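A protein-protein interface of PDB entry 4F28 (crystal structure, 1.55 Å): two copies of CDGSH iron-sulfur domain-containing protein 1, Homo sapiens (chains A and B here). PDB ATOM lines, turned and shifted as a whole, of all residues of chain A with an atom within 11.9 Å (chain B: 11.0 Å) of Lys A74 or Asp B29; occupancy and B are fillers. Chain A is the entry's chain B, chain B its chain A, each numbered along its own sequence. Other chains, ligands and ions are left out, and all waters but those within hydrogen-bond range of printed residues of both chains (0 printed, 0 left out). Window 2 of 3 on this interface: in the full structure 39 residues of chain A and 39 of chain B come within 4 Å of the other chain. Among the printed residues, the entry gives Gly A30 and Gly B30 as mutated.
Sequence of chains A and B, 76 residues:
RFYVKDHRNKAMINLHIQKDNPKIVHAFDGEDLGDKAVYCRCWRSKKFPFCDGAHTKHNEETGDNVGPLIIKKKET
Among the printed residues, pairs that only touch across the chains: Ile A70 with Ala B27 (3.3 Å), Ile A71 with Phe B28 (3.3 Å), Leu A69 with His B26 (3.5 Å), Leu A69 with Tyr B39 (3.5 Å), Leu A69 with Phe B28 (3.7 Å), Lys A74 with Asp B29 (3.7 Å), Tyr A39 with Ile B71 (3.7 Å), Ile A71 with Gly B30 (3.8 Å), Ile A71 with Tyr B39 (3.8 Å) and Gly A30 with Ile B71 (3.9 Å).
N of Gly B30 lies within hydrogen-bond range of O of Lys A72 (2.7 Å).
The backbone carbonyl oxygen (O) of Phe B28 lies within hydrogen-bond range of the backbone NH (N) of Lys A72 (2.9 Å).
The backbone carbonyl oxygen (O) of Ile A70 lies within hydrogen-bond range of the backbone NH (N) of Phe B28.
O of His B26 sits at hydrogen-bond distance from N of Ile A70, at 2.7 Å.
The backbone carbonyl oxygen (O) of Pro A68 is in hydrogen-bond range of the backbone NH (N) of His B26 (3.2 Å).
NZ of Lys A72 lies within salt-bridge range of OD1 of Asp B29, at 2.8 Å.
Of the 14 printed residues of chain B, 7 touch a printed residue of chain A.
Hydrophobic or aromatic side chains of chain B within 4 Å of the printed part of chain A: His B26, Ala B27, Phe B28, Tyr B39 and Ile B71.
Of the 17 printed residues of chain A, 8 touch a printed residue of chain B.
Gly A30 touches Ile B71, and with the chains exchanged Ile A71 touches Gly B30.
Tyr A39 touches Ile B71, and with the chains exchanged Ile A71 touches Tyr B39.
9 positions are printed for both chains.
Of the 16 pairs that touch across the chains among the printed residues, 4 have their exchanged pair printed and touching as well.
Gly A34 touches none of the printed residues of chain B.
Printed residues of chain B within 4 Å of Tyr A39: Ile B71 (3.7 Å).
Ile A71 touches three residues of chain B.
No residue of chain B comes within 4 Å of Lys A73.
Of chain B, only Asp B29 (3.7 Å) comes within 4 Å of Lys A74.
Of the printed residues of chain A, Ala B27 touches Ile A70 (3.3 Å).
Of chain A, only Leu A69, Ile A70, Ile A71 and Lys A72 come within 4 Å of Phe B28.
Of chain A, only Lys A72 and Lys A74 come within 4 Å of Asp B29.
Of the printed residues of chain A, Gly B30 touches Ile A71 (3.8 Å) and Lys A72 (2.7 Å).
No residue of chain A comes within 4 Å of Glu B31.
No residue of chain A comes within 4 Å of Leu B33.
Of the printed residues of chain A, Ile B71 touches Gly A30 (3.9 Å) and Tyr A39 (3.7 Å).
The nearest residue of chain A that does not touch Asp B29 is Lys A73 (4.4 Å).
The backbone NH (N) of Ala A37 is in hydrogen-bond range of the backbone carbonyl oxygen (O) of Ile A71, 2.8 Å away.
The backbone carbonyl oxygen (O) of Leu A69 is in hydrogen-bond range of the backbone NH (N) of Tyr A39, 2.8 Å away.
N of Ala B37 lies within hydrogen-bond range of O of Ile B71, at 2.8 Å.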
ATOM      1  N   ASP A  29     -17.420 -11.781 -21.322  1.00  0.00           N
ATOM      2  CA  ASP A  29     -18.306 -12.358 -22.336  1.00  0.00           C
ATOM      3  C   ASP A  29     -18.518 -11.285 -23.389  1.00  0.00           C
ATOM      4  O   ASP A  29     -18.893 -10.164 -23.035  1.00  0.00           O
ATOM      5  CB  ASP A  29     -19.644 -12.840 -21.735  1.00  0.00           C
ATOM      6  CG  ASP A  29     -19.511 -13.959 -20.707  1.00  0.00           C
ATOM      7  OD1 ASP A  29     -18.908 -15.003 -21.040  1.00  0.00           O
ATOM      8  OD2 ASP A  29     -20.044 -13.802 -19.580  1.00  0.00           O
ATOM      9  N   GLY A  30     -18.219 -11.614 -24.646  1.00  0.00           N
ATOM     10  CA  GLY A  30     -18.328 -10.707 -25.788  1.00  0.00           C
ATOM     11  C   GLY A  30     -19.672 -10.017 -25.948  1.00  0.00           C
ATOM     12  O   GLY A  30     -19.725  -8.840 -26.317  1.00  0.00           O
ATOM     13  N   GLU A  31     -20.766 -10.741 -25.642  1.00  0.00           N
ATOM     14  CA  GLU A  31     -22.133 -10.219 -25.724  1.00  0.00           C
ATOM     15  C   GLU A  31     -22.387  -9.139 -24.654  1.00  0.00           C
ATOM     16  O   GLU A  31     -23.233  -8.268 -24.863  1.00  0.00           O
ATOM     17  CB  GLU A  31     -23.147 -11.362 -25.572  1.00  0.00           C
ATOM     18  N   LEU A  33     -20.156  -6.846 -23.670  1.00  0.00           N
ATOM     19  CA  LEU A  33     -19.427  -5.608 -23.959  1.00  0.00           C
ATOM     20  C   LEU A  33     -20.344  -4.637 -24.674  1.00  0.00           C
ATOM     21  O   LEU A  33     -21.187  -5.062 -25.474  1.00  0.00           O
ATOM     22  CB  LEU A  33     -18.163  -5.834 -24.824  1.00  0.00           C
ATOM     23  CG  LEU A  33     -17.263  -7.053 -24.600  1.00  0.00           C
ATOM     24  CD1 LEU A  33     -16.020  -6.965 -25.486  1.00  0.00           C
ATOM     25  CD2 LEU A  33     -16.851  -7.200 -23.146  1.00  0.00           C
ATOM     26  N   GLY A  34     -20.138  -3.345 -24.435  1.00  0.00           N
ATOM     27  CA  GLY A  34     -20.894  -2.298 -25.114  1.00  0.00           C
ATOM     28  C   GLY A  34     -20.494  -2.142 -26.577  1.00  0.00           C
ATOM     29  O   GLY A  34     -19.895  -3.050 -27.165  1.00  0.00           O
ATOM     30  N   ASP A  35     -20.806  -0.981 -27.177  1.00  0.00           N
ATOM     31  CA  ASP A  35     -20.477  -0.703 -28.579  1.00  0.00           C
ATOM     32  C   ASP A  35     -18.958  -0.569 -28.808  1.00  0.00           C
ATOM     33  O   ASP A  35     -18.485  -0.855 -29.913  1.00  0.00           O
ATOM     34  CB  ASP A  35     -21.199   0.563 -29.069  1.00  0.00           C
ATOM     35  N   LYS A  36     -18.204  -0.129 -27.780  1.00  0.00           N
ATOM     36  CA  LYS A  36     -16.753   0.031 -27.884  1.00  0.00           C
ATOM     37  C   LYS A  36     -16.095  -0.130 -26.523  1.00  0.00           C
ATOM     38  O   LYS A  36     -16.358   0.651 -25.605  1.00  0.00           O
ATOM     39  CB  LYS A  36     -16.388   1.397 -28.502  1.00  0.00           C
ATOM     40  CG  LYS A  36     -14.916   1.549 -28.879  1.00  0.00           C
ATOM     41  CD  LYS A  36     -14.659   2.897 -29.540  1.00  0.00           C
ATOM     42  CE  LYS A  36     -13.205   3.083 -29.895  1.00  0.00           C
ATOM     43  NZ  LYS A  36     -13.032   3.999 -31.058  1.00  0.00           N
ATOM     44  N   ALA A  37     -15.251  -1.159 -26.393  1.00  0.00           N
ATOM     45  CA  ALA A  37     -14.488  -1.420 -25.175  1.00  0.00           C
ATOM     46  C   ALA A  37     -13.010  -1.237 -25.491  1.00  0.00           C
ATOM     47  O   ALA A  37     -12.519  -1.793 -26.482  1.00  0.00           O
ATOM     48  CB  ALA A  37     -14.772  -2.819 -24.643  1.00  0.00           C
ATOM     49  N   VAL A  38     -12.325  -0.396 -24.688  1.00  0.00           N
ATOM     50  CA  VAL A  38     -10.916  -0.056 -24.906  1.00  0.00           C
ATOM     51  C   VAL A  38     -10.134  -0.569 -23.704  1.00  0.00           C
ATOM     52  O   VAL A  38     -10.276  -0.044 -22.589  1.00  0.00           O
ATOM     53  CB  VAL A  38     -10.722   1.476 -25.177  1.00  0.00           C
ATOM     54  CG1 VAL A  38      -9.293   1.786 -25.585  1.00  0.00           C
ATOM     55  CG2 VAL A  38     -11.693   1.988 -26.237  1.00  0.00           C
ATOM     56  N   TYR A  39      -9.307  -1.609 -23.931  1.00  0.00           N
ATOM     57  CA  TYR A  39      -8.574  -2.296 -22.874  1.00  0.00           C
ATOM     58  C   TYR A  39      -7.118  -1.855 -22.758  1.00  0.00           C
ATOM     59  O   TYR A  39      -6.390  -1.763 -23.742  1.00  0.00           O
ATOM     60  CB  TYR A  39      -8.665  -3.803 -23.085  1.00  0.00           C
ATOM     61  CG  TYR A  39     -10.085  -4.324 -22.981  1.00  0.00           C
ATOM     62  CD1 TYR A  39     -10.668  -4.570 -21.739  1.00  0.00           C
ATOM     63  CD2 TYR A  39     -10.818  -4.642 -24.121  1.00  0.00           C
ATOM     64  CE1 TYR A  39     -11.962  -5.067 -21.636  1.00  0.00           C
ATOM     65  CE2 TYR A  39     -12.108  -5.152 -24.032  1.00  0.00           C
ATOM     66  CZ  TYR A  39     -12.682  -5.351 -22.784  1.00  0.00           C
ATOM     67  OH  TYR A  39     -13.945  -5.876 -22.695  1.00  0.00           O
ATOM     68  N   PRO A  68      -3.608   0.560 -26.522  1.00  0.00           N
ATOM     69  CA  PRO A  68      -4.660  -0.370 -26.103  1.00  0.00           C
ATOM     70  C   PRO A  68      -5.158  -1.342 -27.177  1.00  0.00           C
ATOM     71  O   PRO A  68      -4.767  -1.302 -28.356  1.00  0.00           O
ATOM     72  CB  PRO A  68      -5.790   0.584 -25.703  1.00  0.00           C
ATOM     73  CG  PRO A  68      -5.627   1.740 -26.668  1.00  0.00           C
ATOM     74  CD  PRO A  68      -4.148   1.931 -26.679  1.00  0.00           C
ATOM     75  N   LEU A  69      -6.049  -2.239 -26.707  1.00  0.00           N
ATOM     76  CA  LEU A  69      -6.789  -3.209 -27.502  1.00  0.00           C
ATOM     77  C   LEU A  69      -8.251  -2.746 -27.540  1.00  0.00           C
ATOM     78  O   LEU A  69      -8.874  -2.539 -26.486  1.00  0.00           O
ATOM     79  CB  LEU A  69      -6.668  -4.607 -26.902  1.00  0.00           C
ATOM     80  CG  LEU A  69      -7.511  -5.701 -27.582  1.00  0.00           C
ATOM     81  CD1 LEU A  69      -6.835  -6.209 -28.867  1.00  0.00           C
ATOM     82  CD2 LEU A  69      -7.800  -6.811 -26.659  1.00  0.00           C
ATOM     83  N   ILE A  70      -8.790  -2.592 -28.739  1.00  0.00           N
ATOM     84  CA  ILE A  70     -10.160  -2.126 -28.940  1.00  0.00           C
ATOM     85  C   ILE A  70     -11.047  -3.254 -29.460  1.00  0.00           C
ATOM     86  O   ILE A  70     -10.689  -3.910 -30.430  1.00  0.00           O
ATOM     87  CB  ILE A  70     -10.208  -0.898 -29.890  1.00  0.00           C
ATOM     88  CG1 ILE A  70      -9.370   0.294 -29.338  1.00  0.00           C
ATOM     89  CG2 ILE A  70     -11.670  -0.462 -30.197  1.00  0.00           C
ATOM     90  CD1 ILE A  70      -9.046   1.390 -30.408  1.00  0.00           C
ATOM     91  N   ILE A  71     -12.182  -3.501 -28.783  1.00  0.00           N
ATOM     92  CA  ILE A  71     -13.211  -4.441 -29.238  1.00  0.00           C
ATOM     93  C   ILE A  71     -14.439  -3.570 -29.506  1.00  0.00           C
ATOM     94  O   ILE A  71     -14.954  -2.925 -28.581  1.00  0.00           O
ATOM     95  CB  ILE A  71     -13.491  -5.644 -28.292  1.00  0.00           C
ATOM     96  CG1 ILE A  71     -12.195  -6.397 -27.841  1.00  0.00           C
ATOM     97  CG2 ILE A  71     -14.511  -6.610 -28.928  1.00  0.00           C
ATOM     98  CD1 ILE A  71     -11.337  -7.173 -28.963  1.00  0.00           C
ATOM     99  N   LYS A  72     -14.870  -3.504 -30.767  1.00  0.00           N
ATOM    100  CA  LYS A  72     -15.973  -2.629 -31.154  1.00  0.00           C
ATOM    101  C   LYS A  72     -17.103  -3.367 -31.873  1.00  0.00           C
ATOM    102  O   LYS A  72     -16.959  -4.532 -32.252  1.00  0.00           O
ATOM    103  CB  LYS A  72     -15.446  -1.476 -32.027  1.00  0.00           C
ATOM    104  CG  LYS A  72     -14.629  -1.911 -33.246  1.00  0.00           C
ATOM    105  CD  LYS A  72     -13.898  -0.743 -33.891  1.00  0.00           C
ATOM    106  CE  LYS A  72     -13.180  -1.165 -35.151  1.00  0.00           C
ATOM    107  NZ  LYS A  72     -14.120  -1.365 -36.291  1.00  0.00           N
ATOM    108  N   LYS A  73     -18.242  -2.679 -32.019  1.00  0.00           N
ATOM    109  CA  LYS A  73     -19.398  -3.187 -32.743  1.00  0.00           C
ATOM    110  C   LYS A  73     -19.265  -2.709 -34.188  1.00  0.00           C
ATOM    111  O   LYS A  73     -18.885  -1.555 -34.408  1.00  0.00           O
ATOM    112  CB  LYS A  73     -20.707  -2.718 -32.083  1.00  0.00           C
ATOM    113  CG  LYS A  73     -21.905  -3.599 -32.410  1.00  0.00           C
ATOM    114  CD  LYS A  73     -23.150  -3.180 -31.639  1.00  0.00           C
ATOM    115  N   LYS A  74     -19.502  -3.610 -35.165  1.00  0.00           N
ATOM    116  CA  LYS A  74     -19.406  -3.356 -36.615  1.00  0.00           C
ATOM    117  C   LYS A  74     -20.190  -2.118 -37.057  1.00  0.00           C
ATOM    118  O   LYS A  74     -19.678  -1.321 -37.842  1.00  0.00           O
ATOM    119  CB  LYS A  74     -19.898  -4.569 -37.412  1.00  0.00           C
ATOM    120  CG  LYS A  74     -18.845  -5.643 -37.593  1.00  0.00           C
ATOM    121  N   HIS B  26      -4.502  -2.259 -31.428  1.00  0.00           N
ATOM    122  CA  HIS B  26      -5.196  -3.287 -32.203  1.00  0.00           C
ATOM    123  C   HIS B  26      -6.687  -3.059 -32.015  1.00  0.00           C
ATOM    124  O   HIS B  26      -7.121  -2.731 -30.911  1.00  0.00           O
ATOM    125  CB  HIS B  26      -4.793  -4.711 -31.815  1.00  0.00           C
ATOM    126  CG  HIS B  26      -3.411  -5.071 -32.244  1.00  0.00           C
ATOM    127  ND1 HIS B  26      -2.302  -4.734 -31.474  1.00  0.00           N
ATOM    128  CD2 HIS B  26      -2.996  -5.716 -33.359  1.00  0.00           C
ATOM    129  CE1 HIS B  26      -1.251  -5.173 -32.159  1.00  0.00           C
ATOM    130  NE2 HIS B  26      -1.619  -5.761 -33.303  1.00  0.00           N
ATOM    131  N   ALA B  27      -7.456  -3.183 -33.100  1.00  0.00           N
ATOM    132  CA  ALA B  27      -8.900  -2.985 -33.059  1.00  0.00           C
ATOM    133  C   ALA B  27      -9.580  -4.108 -33.809  1.00  0.00           C
ATOM    134  O   ALA B  27      -9.273  -4.387 -34.994  1.00  0.00           O
ATOM    135  CB  ALA B  27      -9.271  -1.619 -33.652  1.00  0.00           C
ATOM    136  N   PHE B  28     -10.486  -4.784 -33.096  1.00  0.00           N
ATOM    137  CA  PHE B  28     -11.237  -5.908 -33.656  1.00  0.00           C
ATOM    138  C   PHE B  28     -12.727  -5.687 -33.507  1.00  0.00           C
ATOM    139  O   PHE B  28     -13.176  -5.114 -32.510  1.00  0.00           O
ATOM    140  CB  PHE B  28     -10.841  -7.217 -32.944  1.00  0.00           C
ATOM    141  CG  PHE B  28      -9.390  -7.620 -33.114  1.00  0.00           C
ATOM    142  CD1 PHE B  28      -8.977  -8.330 -34.233  1.00  0.00           C
ATOM    143  CD2 PHE B  28      -8.442  -7.330 -32.122  1.00  0.00           C
ATOM    144  CE1 PHE B  28      -7.634  -8.716 -34.386  1.00  0.00           C
ATOM    145  CE2 PHE B  28      -7.102  -7.726 -32.267  1.00  0.00           C
ATOM    146  CZ  PHE B  28      -6.700  -8.397 -33.408  1.00  0.00           C
ATOM    147  N   ASP B  29     -13.500  -6.171 -34.487  1.00  0.00           N
ATOM    148  CA  ASP B  29     -14.959  -6.150 -34.427  1.00  0.00           C
ATOM    149  C   ASP B  29     -15.381  -7.353 -33.610  1.00  0.00           C
ATOM    150  O   ASP B  29     -14.933  -8.467 -33.899  1.00  0.00           O
ATOM    151  CB  ASP B  29     -15.581  -6.190 -35.845  1.00  0.00           C
ATOM    152  CG  ASP B  29     -15.273  -4.989 -36.715  1.00  0.00           C
ATOM    153  OD1 ASP B  29     -15.513  -3.841 -36.260  1.00  0.00           O
ATOM    154  OD2 ASP B  29     -14.862  -5.192 -37.878  1.00  0.00           O
ATOM    155  N   GLY B  30     -16.180  -7.115 -32.567  1.00  0.00           N
ATOM    156  CA  GLY B  30     -16.674  -8.142 -31.653  1.00  0.00           C
ATOM    157  C   GLY B  30     -17.354  -9.327 -32.312  1.00  0.00           C
ATOM    158  O   GLY B  30     -17.176 -10.461 -31.864  1.00  0.00           O
ATOM    159  N   GLU B  31     -18.096  -9.078 -33.420  1.00  0.00           N
ATOM    160  CA  GLU B  31     -18.792 -10.131 -34.170  1.00  0.00           C
ATOM    161  C   GLU B  31     -17.793 -11.067 -34.875  1.00  0.00           C
ATOM    162  O   GLU B  31     -18.115 -12.234 -35.114  1.00  0.00           O
ATOM    163  CB  GLU B  31     -19.749  -9.503 -35.195  1.00  0.00           C
ATOM    164  N   ASP B  32     -16.574 -10.561 -35.167  1.00  0.00           N
ATOM    165  CA  ASP B  32     -15.525 -11.315 -35.861  1.00  0.00           C
ATOM    166  C   ASP B  32     -14.684 -12.193 -34.935  1.00  0.00           C
ATOM    167  O   ASP B  32     -13.854 -12.963 -35.428  1.00  0.00           O
ATOM    168  CB  ASP B  32     -14.604 -10.375 -36.639  1.00  0.00           C
ATOM    169  CG  ASP B  32     -15.247  -9.768 -37.866  1.00  0.00           C
ATOM    170  OD1 ASP B  32     -16.349 -10.220 -38.247  1.00  0.00           O
ATOM    171  OD2 ASP B  32     -14.662  -8.841 -38.429  1.00  0.00           O
ATOM    172  N   LEU B  33     -14.843 -12.038 -33.611  1.00  0.00           N
ATOM    173  CA  LEU B  33     -14.107 -12.855 -32.652  1.00  0.00           C
ATOM    174  C   LEU B  33     -14.686 -14.258 -32.589  1.00  0.00           C
ATOM    175  O   LEU B  33     -15.907 -14.423 -32.694  1.00  0.00           O
ATOM    176  CB  LEU B  33     -14.136 -12.214 -31.258  1.00  0.00           C
ATOM    177  CG  LEU B  33     -12.937 -11.313 -30.912  1.00  0.00           C
ATOM    178  CD1 LEU B  33     -12.938 -10.009 -31.709  1.00  0.00           C
ATOM    179  CD2 LEU B  33     -12.924 -10.986 -29.447  1.00  0.00           C
ATOM    180  N   GLY B  34     -13.811 -15.248 -32.392  1.00  0.00           N
ATOM    181  CA  GLY B  34     -14.195 -16.650 -32.238  1.00  0.00           C
ATOM    182  C   GLY B  34     -14.812 -16.924 -30.876  1.00  0.00           C
ATOM    183  O   GLY B  34     -15.192 -15.983 -30.170  1.00  0.00           O
ATOM    184  N   ASP B  35     -14.892 -18.207 -30.475  1.00  0.00           N
ATOM    185  CA  ASP B  35     -15.473 -18.584 -29.185  1.00  0.00           C
ATOM    186  C   ASP B  35     -14.607 -18.133 -27.997  1.00  0.00           C
ATOM    187  O   ASP B  35     -15.149 -17.874 -26.918  1.00  0.00           O
ATOM    188  CB  ASP B  35     -15.715 -20.099 -29.104  1.00  0.00           C
ATOM    189  N   ALA B  37     -10.917 -15.655 -27.453  1.00  0.00           N
ATOM    190  CA  ALA B  37      -9.741 -14.916 -27.916  1.00  0.00           C
ATOM    191  C   ALA B  37      -8.939 -14.500 -26.698  1.00  0.00           C
ATOM    192  O   ALA B  37      -9.520 -13.971 -25.744  1.00  0.00           O
ATOM    193  CB  ALA B  37     -10.145 -13.696 -28.743  1.00  0.00           C
ATOM    194  N   TYR B  39      -5.761 -12.322 -25.451  1.00  0.00           N
ATOM    195  CA  TYR B  39      -4.905 -11.211 -25.856  1.00  0.00           C
ATOM    196  C   TYR B  39      -3.746 -10.957 -24.890  1.00  0.00           C
ATOM    197  O   TYR B  39      -3.921 -10.939 -23.673  1.00  0.00           O
ATOM    198  CB  TYR B  39      -5.764  -9.959 -26.024  1.00  0.00           C
ATOM    199  CG  TYR B  39      -6.778 -10.093 -27.139  1.00  0.00           C
ATOM    200  CD1 TYR B  39      -6.421  -9.854 -28.465  1.00  0.00           C
ATOM    201  CD2 TYR B  39      -8.121 -10.334 -26.862  1.00  0.00           C
ATOM    202  CE1 TYR B  39      -7.354  -9.964 -29.497  1.00  0.00           C
ATOM    203  CE2 TYR B  39      -9.071 -10.408 -27.881  1.00  0.00           C
ATOM    204  CZ  TYR B  39      -8.677 -10.248 -29.199  1.00  0.00           C
ATOM    205  OH  TYR B  39      -9.593 -10.316 -30.227  1.00  0.00           O
ATOM    206  N   PHE B  50      -1.835 -11.765 -29.727  1.00  0.00           N
ATOM    207  CA  PHE B  50      -2.375 -12.907 -28.997  1.00  0.00           C
ATOM    208  C   PHE B  50      -1.360 -13.428 -27.985  1.00  0.00           C
ATOM    209  O   PHE B  50      -0.147 -13.326 -28.208  1.00  0.00           O
ATOM    210  CB  PHE B  50      -2.825 -14.011 -29.980  1.00  0.00           C
ATOM    211  CG  PHE B  50      -3.885 -13.509 -30.944  1.00  0.00           C
ATOM    212  CD1 PHE B  50      -5.198 -13.302 -30.519  1.00  0.00           C
ATOM    213  CD2 PHE B  50      -3.551 -13.157 -32.246  1.00  0.00           C
ATOM    214  CE1 PHE B  50      -6.162 -12.784 -31.391  1.00  0.00           C
ATOM    215  CE2 PHE B  50      -4.518 -12.638 -33.118  1.00  0.00           C
ATOM    216  CZ  PHE B  50      -5.815 -12.453 -32.686  1.00  0.00           C
ATOM    217  N   ILE B  71     -11.564 -12.695 -24.131  1.00  0.00           N
ATOM    218  CA  ILE B  71     -12.907 -12.372 -24.605  1.00  0.00           C
ATOM    219  C   ILE B  71     -13.484 -13.706 -25.052  1.00  0.00           C
ATOM    220  O   ILE B  71     -12.915 -14.345 -25.939  1.00  0.00           O
ATOM    221  CB  ILE B  71     -12.967 -11.265 -25.722  1.00  0.00           C
ATOM    222  CG1 ILE B  71     -12.172  -9.966 -25.356  1.00  0.00           C
ATOM    223  CG2 ILE B  71     -14.436 -10.955 -26.094  1.00  0.00           C
ATOM    224  CD1 ILE B  71     -12.694  -9.106 -24.121  1.00  0.00           C
